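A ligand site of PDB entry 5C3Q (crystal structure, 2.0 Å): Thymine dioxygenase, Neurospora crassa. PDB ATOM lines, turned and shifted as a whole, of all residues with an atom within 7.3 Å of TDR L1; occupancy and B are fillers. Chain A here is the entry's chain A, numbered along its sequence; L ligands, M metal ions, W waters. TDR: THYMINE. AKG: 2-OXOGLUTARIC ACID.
Water W1 lies within hydrogen-bond range of the side-chain carboxylate (OE1) of Glu 124, a nitrogen (N1) of TDR L1, the side-chain amide oxygen (OD1) of Asn 89 and the guanidinium group (NH2) of Arg 192.
Water W2 bridges O2 of TDR L1 (2.7 Å) and ND2 of Asn 296 (2.8 Å).
Water W3 lies within hydrogen-bond range of N3 of TDR L1 (2.8 Å), OD1 of Asn 296 (2.9 Å) and N of Gly 220 (3.3 Å).
The side-chain amide oxygen of Asn 89 lies within hydrogen-bond range of the indole nitrogen of Trp 83.
The side-chain hydroxyl (OG1) of Thr 223 sits at hydrogen-bond distance from the side-chain carboxylate (OD2) of Asp 218 (2.6 Å).
The backbone carbonyl oxygen (O) of Asp 218 sits at hydrogen-bond distance from the backbone NH (N) of Asp 258, 2.8 Å away.
ND2 of Asn 255 lies within hydrogen-bond range of OD2 of Asp 218 (3.1 Å).
The backbone carbonyl oxygen of Ile 190 is in hydrogen-bond range of the backbone NH of Phe 294, at 2.8 Å.
The side-chain carboxylate (OE1) of Glu 124 is in salt-bridge range of the guanidinium group (NE) of Arg 192 (2.8 Å).
Arg 192 touches TDR L1.
His 216 touches TDR L1 (CD2 to CM5, 3.9 Å).
CA of Asp 218 touches O4 of TDR L1, 3.4 Å away.
CG of Phe 294 touches N3 of TDR L1, at 3.5 Å.
Leu 331 touches TDR L1 (CD2 to O2, 3.8 Å).
Hydrophobic or aromatic side chains within 4 Å of TDR L1: His 216, Tyr 219, Phe 294 and Leu 331.
Seven residues have an atom within 4 Å of TDR L1: Asn 89, Arg 192, His 216, Asp 218, Tyr 219, Phe 294 and Leu 331.
The nearest printed residue that does not touch TDR L1 is Glu 124 (4.1 Å).
The backbone NH (N) of Tyr 219 is in hydrogen-bond range of an oxygen (O4) of TDR L1 (2.8 Å).
ND2 of Asn 89 is in hydrogen-bond range of O2 of TDR L1 (3.0 Å).
NH1 of Arg 192 is in salt-bridge range of O2 of AKG L2, at 2.9 Å.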
ATOM      1  N   TRP A  83      43.503  32.067 -27.785  1.00  0.00           N
ATOM      2  CA  TRP A  83      42.956  32.069 -26.432  1.00  0.00           C
ATOM      3  C   TRP A  83      44.132  32.067 -25.464  1.00  0.00           C
ATOM      4  O   TRP A  83      45.073  31.303 -25.637  1.00  0.00           O
ATOM      5  CB  TRP A  83      42.106  30.821 -26.229  1.00  0.00           C
ATOM      6  CG  TRP A  83      41.127  30.825 -25.090  1.00  0.00           C
ATOM      7  CD1 TRP A  83      39.827  31.246 -25.131  1.00  0.00           C
ATOM      8  CD2 TRP A  83      41.347  30.342 -23.752  1.00  0.00           C
ATOM      9  NE1 TRP A  83      39.232  31.071 -23.910  1.00  0.00           N
ATOM     10  CE2 TRP A  83      40.137  30.512 -23.050  1.00  0.00           C
ATOM     11  CE3 TRP A  83      42.450  29.777 -23.098  1.00  0.00           C
ATOM     12  CZ2 TRP A  83      39.999  30.155 -21.705  1.00  0.00           C
ATOM     13  CZ3 TRP A  83      42.313  29.426 -21.761  1.00  0.00           C
ATOM     14  CH2 TRP A  83      41.091  29.607 -21.077  1.00  0.00           C
ATOM     15  N   ASN A  89      39.153  34.686 -21.353  1.00  0.00           N
ATOM     16  CA  ASN A  89      38.217  33.812 -22.077  1.00  0.00           C
ATOM     17  C   ASN A  89      37.891  34.325 -23.489  1.00  0.00           C
ATOM     18  O   ASN A  89      36.743  34.298 -23.927  1.00  0.00           O
ATOM     19  CB  ASN A  89      36.931  33.619 -21.261  1.00  0.00           C
ATOM     20  CG  ASN A  89      36.136  32.397 -21.687  1.00  0.00           C
ATOM     21  OD1 ASN A  89      36.683  31.462 -22.272  1.00  0.00           O
ATOM     22  ND2 ASN A  89      34.843  32.392 -21.388  1.00  0.00           N
ATOM     23  N   GLU A 124      36.402  33.006 -29.614  1.00  0.00           N
ATOM     24  CA  GLU A 124      35.537  33.614 -28.611  1.00  0.00           C
ATOM     25  C   GLU A 124      35.738  35.134 -28.472  1.00  0.00           C
ATOM     26  O   GLU A 124      36.862  35.632 -28.391  1.00  0.00           O
ATOM     27  CB  GLU A 124      35.729  32.905 -27.276  1.00  0.00           C
ATOM     28  CG  GLU A 124      35.092  31.521 -27.306  1.00  0.00           C
ATOM     29  CD  GLU A 124      35.569  30.609 -26.199  1.00  0.00           C
ATOM     30  OE1 GLU A 124      34.709  29.933 -25.592  1.00  0.00           O
ATOM     31  OE2 GLU A 124      36.790  30.565 -25.953  1.00  0.00           O
ATOM     32  N   ASN A 189      28.994  38.576 -21.543  1.00  0.00           N
ATOM     33  CA  ASN A 189      28.679  37.374 -22.298  1.00  0.00           C
ATOM     34  C   ASN A 189      29.852  36.985 -23.203  1.00  0.00           C
ATOM     35  O   ASN A 189      30.762  37.786 -23.424  1.00  0.00           O
ATOM     36  CB  ASN A 189      27.429  37.628 -23.122  1.00  0.00           C
ATOM     37  CG  ASN A 189      26.254  38.089 -22.262  1.00  0.00           C
ATOM     38  OD1 ASN A 189      26.095  37.633 -21.127  1.00  0.00           O
ATOM     39  ND2 ASN A 189      25.454  38.999 -22.795  1.00  0.00           N
ATOM     40  N   ILE A 190      29.826  35.753 -23.701  1.00  0.00           N
ATOM     41  CA  ILE A 190      30.872  35.276 -24.597  1.00  0.00           C
ATOM     42  C   ILE A 190      30.244  34.747 -25.892  1.00  0.00           C
ATOM     43  O   ILE A 190      29.379  33.865 -25.859  1.00  0.00           O
ATOM     44  CB  ILE A 190      31.746  34.185 -23.946  1.00  0.00           C
ATOM     45  CG1 ILE A 190      32.549  34.766 -22.774  1.00  0.00           C
ATOM     46  CG2 ILE A 190      32.697  33.549 -24.964  1.00  0.00           C
ATOM     47  CD1 ILE A 190      33.648  35.734 -23.154  1.00  0.00           C
ATOM     48  N   ARG A 192      30.842  32.612 -28.866  1.00  0.00           N
ATOM     49  CA  ARG A 192      31.705  31.522 -29.330  1.00  0.00           C
ATOM     50  C   ARG A 192      31.326  31.089 -30.745  1.00  0.00           C
ATOM     51  O   ARG A 192      30.279  30.473 -30.965  1.00  0.00           O
ATOM     52  CB  ARG A 192      31.624  30.325 -28.381  1.00  0.00           C
ATOM     53  CG  ARG A 192      32.514  29.161 -28.787  1.00  0.00           C
ATOM     54  CD  ARG A 192      32.303  27.944 -27.905  1.00  0.00           C
ATOM     55  NE  ARG A 192      33.326  27.820 -26.880  1.00  0.00           N
ATOM     56  CZ  ARG A 192      33.437  26.799 -26.032  1.00  0.00           C
ATOM     57  NH1 ARG A 192      32.564  25.790 -26.063  1.00  0.00           N
ATOM     58  NH2 ARG A 192      34.417  26.791 -25.136  1.00  0.00           N
ATOM     59  N   HIS A 216      28.910  17.873 -21.813  1.00  0.00           N
ATOM     60  CA  HIS A 216      29.130  18.889 -20.804  1.00  0.00           C
ATOM     61  C   HIS A 216      27.824  19.591 -20.455  1.00  0.00           C
ATOM     62  O   HIS A 216      26.808  19.393 -21.133  1.00  0.00           O
ATOM     63  CB  HIS A 216      30.110  19.928 -21.330  1.00  0.00           C
ATOM     64  CG  HIS A 216      29.588  20.673 -22.509  1.00  0.00           C
ATOM     65  ND1 HIS A 216      29.478  20.101 -23.757  1.00  0.00           N
ATOM     66  CD2 HIS A 216      29.087  21.928 -22.626  1.00  0.00           C
ATOM     67  CE1 HIS A 216      28.957  20.979 -24.599  1.00  0.00           C
ATOM     68  NE2 HIS A 216      28.709  22.086 -23.942  1.00  0.00           N
ATOM     69  N   THR A 217      27.860  20.394 -19.401  1.00  0.00           N
ATOM     70  CA  THR A 217      26.836  21.382 -19.134  1.00  0.00           C
ATOM     71  C   THR A 217      27.436  22.761 -19.368  1.00  0.00           C
ATOM     72  O   THR A 217      28.651  22.964 -19.182  1.00  0.00           O
ATOM     73  CB  THR A 217      26.305  21.289 -17.688  1.00  0.00           C
ATOM     74  OG1 THR A 217      27.388  21.405 -16.762  1.00  0.00           O
ATOM     75  CG2 THR A 217      25.583  19.970 -17.455  1.00  0.00           C
ATOM     76  N   ASP A 218      26.603  23.715 -19.792  1.00  0.00           N
ATOM     77  CA  ASP A 218      27.029  25.101 -19.920  1.00  0.00           C
ATOM     78  C   ASP A 218      27.061  25.750 -18.540  1.00  0.00           C
ATOM     79  O   ASP A 218      26.392  25.286 -17.620  1.00  0.00           O
ATOM     80  CB  ASP A 218      26.097  25.881 -20.863  1.00  0.00           C
ATOM     81  CG  ASP A 218      26.240  25.450 -22.322  1.00  0.00           C
ATOM     82  OD1 ASP A 218      27.118  24.637 -22.667  1.00  0.00           O
ATOM     83  OD2 ASP A 218      25.446  25.953 -23.154  1.00  0.00           O
ATOM     84  N   TYR A 219      27.832  26.835 -18.406  1.00  0.00           N
ATOM     85  CA  TYR A 219      28.170  27.388 -17.090  1.00  0.00           C
ATOM     86  C   TYR A 219      27.254  28.516 -16.599  1.00  0.00           C
ATOM     87  O   TYR A 219      27.070  28.660 -15.385  1.00  0.00           O
ATOM     88  CB  TYR A 219      29.599  27.948 -17.088  1.00  0.00           C
ATOM     89  CG  TYR A 219      30.672  27.036 -17.637  1.00  0.00           C
ATOM     90  CD1 TYR A 219      30.583  25.643 -17.525  1.00  0.00           C
ATOM     91  CD2 TYR A 219      31.811  27.569 -18.245  1.00  0.00           C
ATOM     92  CE1 TYR A 219      31.583  24.824 -18.019  1.00  0.00           C
ATOM     93  CE2 TYR A 219      32.811  26.749 -18.739  1.00  0.00           C
ATOM     94  CZ  TYR A 219      32.690  25.388 -18.630  1.00  0.00           C
ATOM     95  OH  TYR A 219      33.687  24.579 -19.116  1.00  0.00           O
ATOM     96  N   GLY A 220      26.711  29.302 -17.531  1.00  0.00           N
ATOM     97  CA  GLY A 220      26.115  30.602 -17.209  1.00  0.00           C
ATOM     98  C   GLY A 220      24.618  30.600 -16.951  1.00  0.00           C
ATOM     99  O   GLY A 220      24.073  29.664 -16.371  1.00  0.00           O
ATOM    100  N   ILE A 222      21.961  31.492 -19.537  1.00  0.00           N
ATOM    101  CA  ILE A 222      21.472  30.760 -20.700  1.00  0.00           C
ATOM    102  C   ILE A 222      22.513  30.776 -21.832  1.00  0.00           C
ATOM    103  O   ILE A 222      23.462  31.568 -21.826  1.00  0.00           O
ATOM    104  CB  ILE A 222      20.126  31.317 -21.252  1.00  0.00           C
ATOM    105  CG1 ILE A 222      20.286  32.726 -21.833  1.00  0.00           C
ATOM    106  CG2 ILE A 222      19.050  31.310 -20.168  1.00  0.00           C
ATOM    107  CD1 ILE A 222      19.040  33.271 -22.488  1.00  0.00           C
ATOM    108  N   THR A 223      22.319  29.883 -22.791  1.00  0.00           N
ATOM    109  CA  THR A 223      23.115  29.869 -23.992  1.00  0.00           C
ATOM    110  C   THR A 223      22.169  29.968 -25.171  1.00  0.00           C
ATOM    111  O   THR A 223      21.147  29.284 -25.212  1.00  0.00           O
ATOM    112  CB  THR A 223      23.969  28.584 -24.113  1.00  0.00           C
ATOM    113  OG1 THR A 223      24.853  28.496 -22.995  1.00  0.00           O
ATOM    114  CG2 THR A 223      24.793  28.588 -25.400  1.00  0.00           C
ATOM    115  N   ASN A 255      19.307  27.018 -24.007  1.00  0.00           N
ATOM    116  CA  ASN A 255      19.396  26.162 -22.836  1.00  0.00           C
ATOM    117  C   ASN A 255      19.901  26.911 -21.620  1.00  0.00           C
ATOM    118  O   ASN A 255      20.735  27.809 -21.731  1.00  0.00           O
ATOM    119  CB  ASN A 255      20.278  24.951 -23.126  1.00  0.00           C
ATOM    120  CG  ASN A 255      21.732  25.320 -23.365  1.00  0.00           C
ATOM    121  OD1 ASN A 255      22.080  25.800 -24.441  1.00  0.00           O
ATOM    122  ND2 ASN A 255      22.586  25.088 -22.377  1.00  0.00           N
ATOM    123  N   GLY A 257      22.073  27.363 -18.233  1.00  0.00           N
ATOM    124  CA  GLY A 257      23.370  26.930 -17.740  1.00  0.00           C
ATOM    125  C   GLY A 257      23.381  26.657 -16.239  1.00  0.00           C
ATOM    126  O   GLY A 257      22.384  26.874 -15.546  1.00  0.00           O
ATOM    127  N   ASP A 258      24.520  26.213 -15.741  1.00  0.00           N
ATOM    128  CA  ASP A 258      24.638  25.773 -14.353  1.00  0.00           C
ATOM    129  C   ASP A 258      24.382  26.876 -13.340  1.00  0.00           C
ATOM    130  O   ASP A 258      23.849  26.611 -12.275  1.00  0.00           O
ATOM    131  CB  ASP A 258      26.011  25.121 -14.117  1.00  0.00           C
ATOM    132  CG  ASP A 258      26.175  23.833 -14.901  1.00  0.00           C
ATOM    133  OD1 ASP A 258      25.133  23.240 -15.280  1.00  0.00           O
ATOM    134  OD2 ASP A 258      27.324  23.396 -15.128  1.00  0.00           O
ATOM    135  N   HIS A 273      24.671  17.969 -22.781  1.00  0.00           N
ATOM    136  CA  HIS A 273      24.585  17.891 -24.222  1.00  0.00           C
ATOM    137  C   HIS A 273      25.962  17.717 -24.849  1.00  0.00           C
ATOM    138  O   HIS A 273      26.983  17.916 -24.195  1.00  0.00           O
ATOM    139  CB  HIS A 273      23.880  19.130 -24.792  1.00  0.00           C
ATOM    140  CG  HIS A 273      24.459  20.425 -24.313  1.00  0.00           C
ATOM    141  ND1 HIS A 273      24.344  20.854 -23.006  1.00  0.00           N
ATOM    142  CD2 HIS A 273      25.163  21.374 -24.972  1.00  0.00           C
ATOM    143  CE1 HIS A 273      24.955  22.022 -22.882  1.00  0.00           C
ATOM    144  NE2 HIS A 273      25.463  22.352 -24.051  1.00  0.00           N
ATOM    145  N   PHE A 294      27.158  32.450 -25.058  1.00  0.00           N
ATOM    146  CA  PHE A 294      27.048  32.157 -23.634  1.00  0.00           C
ATOM    147  C   PHE A 294      26.635  33.414 -22.897  1.00  0.00           C
ATOM    148  O   PHE A 294      27.375  34.405 -22.878  1.00  0.00           O
ATOM    149  CB  PHE A 294      28.378  31.656 -23.077  1.00  0.00           C
ATOM    150  CG  PHE A 294      28.883  30.403 -23.727  1.00  0.00           C
ATOM    151  CD1 PHE A 294      28.132  29.239 -23.680  1.00  0.00           C
ATOM    152  CD2 PHE A 294      30.113  30.378 -24.363  1.00  0.00           C
ATOM    153  CE1 PHE A 294      28.599  28.071 -24.265  1.00  0.00           C
ATOM    154  CE2 PHE A 294      30.581  29.217 -24.956  1.00  0.00           C
ATOM    155  CZ  PHE A 294      29.821  28.057 -24.906  1.00  0.00           C
ATOM    156  N   CYS A 295      25.448  33.388 -22.298  1.00  0.00           N
ATOM    157  CA  CYS A 295      24.976  34.487 -21.486  1.00  0.00           C
ATOM    158  C   CYS A 295      25.309  34.236 -20.018  1.00  0.00           C
ATOM    159  O   CYS A 295      25.165  33.107 -19.521  1.00  0.00           O
ATOM    160  CB  CYS A 295      23.480  34.694 -21.650  1.00  0.00           C
ATOM    161  SG  CYS A 295      22.939  34.875 -23.359  1.00  0.00           S
ATOM    162  N   ASN A 296      25.745  35.294 -19.343  1.00  0.00           N
ATOM    163  CA  ASN A 296      26.109  35.224 -17.933  1.00  0.00           C
ATOM    164  C   ASN A 296      25.471  36.366 -17.151  1.00  0.00           C
ATOM    165  O   ASN A 296      25.213  37.432 -17.707  1.00  0.00           O
ATOM    166  CB  ASN A 296      27.626  35.323 -17.778  1.00  0.00           C
ATOM    167  CG  ASN A 296      28.359  34.159 -18.428  1.00  0.00           C
ATOM    168  OD1 ASN A 296      28.100  33.004 -18.115  1.00  0.00           O
ATOM    169  ND2 ASN A 296      29.288  34.471 -19.320  1.00  0.00           N
ATOM    170  N   LEU A 327      32.465  31.470 -12.604  1.00  0.00           N
ATOM    171  CA  LEU A 327      32.787  31.225 -14.016  1.00  0.00           C
ATOM    172  C   LEU A 327      34.268  30.955 -14.237  1.00  0.00           C
ATOM    173  O   LEU A 327      34.628  30.023 -14.950  1.00  0.00           O
ATOM    174  CB  LEU A 327      32.351  32.390 -14.892  1.00  0.00           C
ATOM    175  CG  LEU A 327      30.870  32.489 -15.219  1.00  0.00           C
ATOM    176  CD1 LEU A 327      30.607  33.794 -15.956  1.00  0.00           C
ATOM    177  CD2 LEU A 327      30.393  31.309 -16.059  1.00  0.00           C
ATOM    178  N   ARG A 330      35.228  27.519 -13.257  1.00  0.00           N
ATOM    179  CA  ARG A 330      34.823  26.536 -14.267  1.00  0.00           C
ATOM    180  C   ARG A 330      35.748  26.575 -15.493  1.00  0.00           C
ATOM    181  O   ARG A 330      36.149  25.548 -16.010  1.00  0.00           O
ATOM    182  CB  ARG A 330      33.370  26.766 -14.718  1.00  0.00           C
ATOM    183  CG  ARG A 330      32.319  26.605 -13.626  1.00  0.00           C
ATOM    184  CD  ARG A 330      32.216  25.188 -13.073  1.00  0.00           C
ATOM    185  NE  ARG A 330      31.865  24.207 -14.103  1.00  0.00           N
ATOM    186  CZ  ARG A 330      30.626  23.922 -14.498  1.00  0.00           C
ATOM    187  NH1 ARG A 330      29.579  24.547 -13.971  1.00  0.00           N
ATOM    188  NH2 ARG A 330      30.430  23.011 -15.433  1.00  0.00           N
ATOM    189  N   LEU A 331      36.069  27.785 -15.950  1.00  0.00           N
ATOM    190  CA  LEU A 331      36.934  27.976 -17.110  1.00  0.00           C
ATOM    191  C   LEU A 331      38.381  27.549 -16.843  1.00  0.00           C
ATOM    192  O   LEU A 331      39.045  27.043 -17.730  1.00  0.00           O
ATOM    193  CB  LEU A 331      36.912  29.431 -17.566  1.00  0.00           C
ATOM    194  CG  LEU A 331      35.589  29.888 -18.170  1.00  0.00           C
ATOM    195  CD1 LEU A 331      35.445  31.405 -18.087  1.00  0.00           C
ATOM    196  CD2 LEU A 331      35.474  29.404 -19.604  1.00  0.00           C
HETATM  197  N1  TDR L   1      32.823  28.612 -22.200  1.00  0.00           N
HETATM  198  C2  TDR L   1      32.000  29.594 -21.524  1.00  0.00           C
HETATM  199  O2  TDR L   1      32.403  30.728 -21.393  1.00  0.00           O
HETATM  200  N3  TDR L   1      30.702  29.207 -21.018  1.00  0.00           N
HETATM  201  C4  TDR L   1      30.218  27.877 -21.170  1.00  0.00           C
HETATM  202  O4  TDR L   1      29.122  27.595 -20.730  1.00  0.00           O
HETATM  203  C5  TDR L   1      31.052  26.873 -21.851  1.00  0.00           C
HETATM  204  CM5 TDR L   1      30.607  25.456 -22.031  1.00  0.00           C
HETATM  205  C6  TDR L   1      32.364  27.268 -22.362  1.00  0.00           C
HETATM  206  C1  AKG L   2      29.127  24.599 -26.684  1.00  0.00           C
HETATM  207  O1  AKG L   2      29.041  24.702 -25.430  1.00  0.00           O
HETATM  208  O2  AKG L   2      29.991  25.208 -27.344  1.00  0.00           O
HETATM  209  C2  AKG L   2      28.181  23.718 -27.388  1.00  0.00           C
HETATM  210  O5  AKG L   2      27.432  22.986 -26.753  1.00  0.00           O
HETATM  211  C3  AKG L   2      28.150  23.727 -28.910  1.00  0.00           C
HETATM  212  C4  AKG L   2      26.994  22.869 -29.434  1.00  0.00           C
HETATM  213  C5  AKG L   2      26.902  22.933 -30.942  1.00  0.00           C
HETATM  214  O3  AKG L   2      25.781  22.703 -31.462  1.00  0.00           O
HETATM  215  O4  AKG L   2      27.916  23.201 -31.630  1.00  0.00           O
HETATM  216 NI    NI M   1      27.242  23.594 -24.617  1.00  0.00          NI
HETATM  217  O   HOH W   1      35.220  29.367 -23.103  1.00  0.00           O
HETATM  218  O   HOH W   2      31.508  32.799 -19.905  1.00  0.00           O
HETATM  219  O   HOH W   3      28.849  30.710 -19.639  1.00  0.00           O
